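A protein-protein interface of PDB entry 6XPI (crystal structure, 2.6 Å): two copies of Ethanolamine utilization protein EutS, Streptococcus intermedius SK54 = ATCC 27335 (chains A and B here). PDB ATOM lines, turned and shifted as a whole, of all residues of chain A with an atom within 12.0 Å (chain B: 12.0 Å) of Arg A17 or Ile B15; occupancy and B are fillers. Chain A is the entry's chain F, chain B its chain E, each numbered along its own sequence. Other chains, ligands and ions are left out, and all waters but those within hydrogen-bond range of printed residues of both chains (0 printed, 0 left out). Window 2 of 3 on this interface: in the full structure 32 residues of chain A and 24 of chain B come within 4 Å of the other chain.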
ATOM      1  N   ASP A  16      13.390  20.010  18.656  1.00  0.00           N
ATOM      2  CA  ASP A  16      13.819  21.015  19.631  1.00  0.00           C
ATOM      3  C   ASP A  16      14.184  20.417  21.004  1.00  0.00           C
ATOM      4  O   ASP A  16      13.869  21.019  22.038  1.00  0.00           O
ATOM      5  CB  ASP A  16      12.769  22.146  19.781  1.00  0.00           C
ATOM      6  CG  ASP A  16      11.368  21.713  20.204  1.00  0.00           C
ATOM      7  OD1 ASP A  16      10.901  20.654  19.723  1.00  0.00           O
ATOM      8  OD2 ASP A  16      10.732  22.449  21.006  1.00  0.00           O
ATOM      9  N   ARG A  17      14.839  19.234  21.014  1.00  0.00           N
ATOM     10  CA  ARG A  17      15.231  18.567  22.254  1.00  0.00           C
ATOM     11  C   ARG A  17      16.694  18.137  22.205  1.00  0.00           C
ATOM     12  O   ARG A  17      17.094  17.423  21.287  1.00  0.00           O
ATOM     13  CB  ARG A  17      14.308  17.369  22.543  1.00  0.00           C
ATOM     14  CG  ARG A  17      14.566  16.737  23.901  1.00  0.00           C
ATOM     15  CD  ARG A  17      13.598  15.631  24.209  1.00  0.00           C
ATOM     16  NE  ARG A  17      12.222  16.111  24.340  1.00  0.00           N
ATOM     17  CZ  ARG A  17      11.596  16.299  25.499  1.00  0.00           C
ATOM     18  NH1 ARG A  17      12.224  16.065  26.647  1.00  0.00           N
ATOM     19  NH2 ARG A  17      10.338  16.724  25.521  1.00  0.00           N
ATOM     20  N   ILE A  18      17.491  18.567  23.188  1.00  0.00           N
ATOM     21  CA  ILE A  18      18.903  18.234  23.203  1.00  0.00           C
ATOM     22  C   ILE A  18      19.420  17.886  24.592  1.00  0.00           C
ATOM     23  O   ILE A  18      19.128  18.581  25.551  1.00  0.00           O
ATOM     24  CB  ILE A  18      19.703  19.387  22.543  1.00  0.00           C
ATOM     25  CG1 ILE A  18      21.216  19.112  22.520  1.00  0.00           C
ATOM     26  CG2 ILE A  18      19.384  20.740  23.178  1.00  0.00           C
ATOM     27  CD1 ILE A  18      21.927  19.995  21.589  1.00  0.00           C
ATOM     28  N   ILE A  19      20.199  16.807  24.699  1.00  0.00           N
ATOM     29  CA  ILE A  19      20.813  16.435  25.962  1.00  0.00           C
ATOM     30  C   ILE A  19      22.001  17.366  26.181  1.00  0.00           C
ATOM     31  O   ILE A  19      22.807  17.556  25.274  1.00  0.00           O
ATOM     32  CB  ILE A  19      21.273  14.970  25.937  1.00  0.00           C
ATOM     33  CG1 ILE A  19      20.111  14.014  25.804  1.00  0.00           C
ATOM     34  CG2 ILE A  19      22.120  14.636  27.161  1.00  0.00           C
ATOM     35  CD1 ILE A  19      20.560  12.636  25.383  1.00  0.00           C
ATOM     36  N   GLN A  20      22.093  17.954  27.364  1.00  0.00           N
ATOM     37  CA  GLN A  20      23.206  18.816  27.686  1.00  0.00           C
ATOM     38  C   GLN A  20      23.962  18.310  28.922  1.00  0.00           C
ATOM     39  O   GLN A  20      23.419  18.218  30.018  1.00  0.00           O
ATOM     40  CB  GLN A  20      22.798  20.297  27.779  1.00  0.00           C
ATOM     41  CG  GLN A  20      21.610  20.591  28.680  1.00  0.00           C
ATOM     42  CD  GLN A  20      22.074  21.446  29.852  1.00  0.00           C
ATOM     43  OE1 GLN A  20      22.062  22.683  29.809  1.00  0.00           O
ATOM     44  NE2 GLN A  20      22.581  20.811  30.912  1.00  0.00           N
ATOM     45  N   GLU A  21      25.212  17.929  28.717  1.00  0.00           N
ATOM     46  CA  GLU A  21      26.078  17.486  29.784  1.00  0.00           C
ATOM     47  C   GLU A  21      26.568  18.749  30.502  1.00  0.00           C
ATOM     48  O   GLU A  21      27.346  19.509  29.955  1.00  0.00           O
ATOM     49  CB  GLU A  21      27.250  16.668  29.210  1.00  0.00           C
ATOM     50  CG  GLU A  21      26.859  15.265  28.766  1.00  0.00           C
ATOM     51  CD  GLU A  21      27.905  14.215  29.113  1.00  0.00           C
ATOM     52  OE1 GLU A  21      29.104  14.460  28.840  1.00  0.00           O
ATOM     53  OE2 GLU A  21      27.530  13.157  29.674  1.00  0.00           O
ATOM     54  N   ILE B  15      18.132  14.017  19.001  1.00  0.00           N
ATOM     55  CA  ILE B  15      18.477  14.091  20.416  1.00  0.00           C
ATOM     56  C   ILE B  15      19.995  13.865  20.603  1.00  0.00           C
ATOM     57  O   ILE B  15      20.456  12.768  20.953  1.00  0.00           O
ATOM     58  CB  ILE B  15      17.554  13.163  21.266  1.00  0.00           C
ATOM     59  CG1 ILE B  15      17.837  13.296  22.764  1.00  0.00           C
ATOM     60  CG2 ILE B  15      17.578  11.705  20.798  1.00  0.00           C
ATOM     61  CD1 ILE B  15      17.535  14.619  23.276  1.00  0.00           C
ATOM     62  N   ASP B  16      20.779  14.910  20.270  1.00  0.00           N
ATOM     63  CA  ASP B  16      22.226  14.839  20.404  1.00  0.00           C
ATOM     64  C   ASP B  16      22.660  15.298  21.825  1.00  0.00           C
ATOM     65  O   ASP B  16      21.816  15.613  22.669  1.00  0.00           O
ATOM     66  CB  ASP B  16      22.975  15.559  19.242  1.00  0.00           C
ATOM     67  CG  ASP B  16      22.716  17.049  19.126  1.00  0.00           C
ATOM     68  OD1 ASP B  16      21.554  17.468  19.334  1.00  0.00           O
ATOM     69  OD2 ASP B  16      23.671  17.797  18.798  1.00  0.00           O
ATOM     70  N   ARG B  17      23.972  15.282  22.092  1.00  0.00           N
ATOM     71  CA  ARG B  17      24.535  15.542  23.396  1.00  0.00           C
ATOM     72  C   ARG B  17      25.642  16.583  23.302  1.00  0.00           C
ATOM     73  O   ARG B  17      26.550  16.466  22.471  1.00  0.00           O
ATOM     74  CB  ARG B  17      25.078  14.211  23.933  1.00  0.00           C
ATOM     75  CG  ARG B  17      25.716  14.280  25.302  1.00  0.00           C
ATOM     76  CD  ARG B  17      26.257  12.927  25.735  1.00  0.00           C
ATOM     77  NE  ARG B  17      25.189  11.938  25.913  1.00  0.00           N
ATOM     78  CZ  ARG B  17      24.627  11.641  27.083  1.00  0.00           C
ATOM     79  NH1 ARG B  17      25.015  12.264  28.191  1.00  0.00           N
ATOM     80  NH2 ARG B  17      23.664  10.730  27.153  1.00  0.00           N
ATOM     81  N   ILE B  18      25.576  17.603  24.161  1.00  0.00           N
ATOM     82  CA  ILE B  18      26.573  18.670  24.141  1.00  0.00           C
ATOM     83  C   ILE B  18      27.034  19.070  25.536  1.00  0.00           C
ATOM     84  O   ILE B  18      26.209  19.234  26.417  1.00  0.00           O
ATOM     85  CB  ILE B  18      26.027  19.868  23.327  1.00  0.00           C
ATOM     86  CG1 ILE B  18      27.010  21.042  23.310  1.00  0.00           C
ATOM     87  CG2 ILE B  18      24.671  20.312  23.820  1.00  0.00           C
ATOM     88  CD1 ILE B  18      26.746  22.004  22.251  1.00  0.00           C
ATOM     89  N   ILE B  19      28.338  19.205  25.746  1.00  0.00           N
ATOM     90  CA  ILE B  19      28.871  19.661  27.017  1.00  0.00           C
ATOM     91  C   ILE B  19      28.629  21.163  27.104  1.00  0.00           C
ATOM     92  O   ILE B  19      28.920  21.893  26.162  1.00  0.00           O
ATOM     93  CB  ILE B  19      30.371  19.330  27.154  1.00  0.00           C
ATOM     94  CG1 ILE B  19      30.584  17.823  27.203  1.00  0.00           C
ATOM     95  CG2 ILE B  19      30.972  19.999  28.375  1.00  0.00           C
ATOM     96  CD1 ILE B  19      31.982  17.402  27.141  1.00  0.00           C
ATOM     97  N   GLN B  20      28.032  21.620  28.203  1.00  0.00           N
ATOM     98  CA  GLN B  20      27.760  23.023  28.433  1.00  0.00           C
ATOM     99  C   GLN B  20      28.451  23.462  29.700  1.00  0.00           C
ATOM    100  O   GLN B  20      28.128  22.977  30.785  1.00  0.00           O
ATOM    101  CB  GLN B  20      26.248  23.302  28.508  1.00  0.00           C
ATOM    102  CG  GLN B  20      25.633  23.449  27.133  1.00  0.00           C
ATOM    103  CD  GLN B  20      24.270  24.091  27.079  1.00  0.00           C
ATOM    104  OE1 GLN B  20      23.232  23.451  27.279  1.00  0.00           O
ATOM    105  NE2 GLN B  20      24.232  25.357  26.721  1.00  0.00           N
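Hydrophobic or aromatic side chains of chain B that line the printed part of chain A: Ile B15, Ile B18 and Ile B19.
Hydrophobic or aromatic side chains of chain A that line the printed part of chain B: Ile A18 and Ile A19.
Ile A19 touches Asp B16, but with the chains exchanged Asp A16 does not touch Ile B19 (15.0 Å).
Ile A19 touches Arg B17, but with the chains exchanged Arg A17 does not touch Ile B19 (12.2 Å).
Ile A19 touches Ile B18, but with the chains exchanged Ile A18 does not touch Ile B19 (7.7 Å).
Gln A20 touches Ile B18, but with the chains exchanged Ile A18 does not touch Gln B20 (6.2 Å).
Of the 14 pairs that touch across the chains among the printed residues, 2 have their exchanged pair printed and touching as well.
No residue of chain B comes within 4 Å of Asp A16.
Ile A18 touches just these residues of chain B: Ile B15, Asp B16 and Ile B18.
Ile A19 touches just these residues of chain B: Ile B15 (3.7 Å), Asp B16 (2.9 Å), Arg B17 (3.3 Å) and Ile B18 (3.0 Å).
Ile B15 touches three residues of chain A.
Of chain A, only Ile A18 and Ile A19 come within 4 Å of Asp B16.
Printed residues of chain A within 4 Å of Arg B17: Ile A19 (3.3 Å) and Glu A21 (3.1 Å).
Printed residues of chain A within 4 Å of Gln B20: Gln A20 and Glu A21.
The nearest residue of chain B that does not touch Arg A17 is Asp B16 (4.6 Å).
The nearest printed residue of chain A that does not touch Ile B18 is Arg A17 (8.4 Å).
NH1 of Arg B17 is in salt-bridge range of OE2 of Glu A21.
The backbone carbonyl oxygen (O) of Ile A19 sits at hydrogen-bond distance from the backbone NH (N) of Ile B18 (3.0 Å).
N of Ile A19 lies within hydrogen-bond range of O of Asp B16.
The backbone NH (N) of Gln B20 sits at hydrogen-bond distance from the backbone carbonyl oxygen (O) of Glu A21 (2.8 Å).
OE1 of Gln A20 sits close to OE1 of Gln B20, at 2.9 Å.
The backbone carbonyl oxygen (O) of Ile B18 is in hydrogen-bond range of the backbone NH (N) of Glu A21, 2.8 Å away.
Among the printed residues, pairs that only touch across the chains: Arg A17 with Ile B15 (3.5 Å), Ile A18 with Ile B15 (3.9 Å), Ile A18 with Asp B16 (3.4 Å), Ile A18 with Ile B18 (3.6 Å), Ile A19 with Ile B15 (3.7 Å), Ile A19 with Arg B17 (3.3 Å), Gln A20 with Ile B18 (3.3 Å) and Glu A21 with Ile B19 (3.3 Å).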
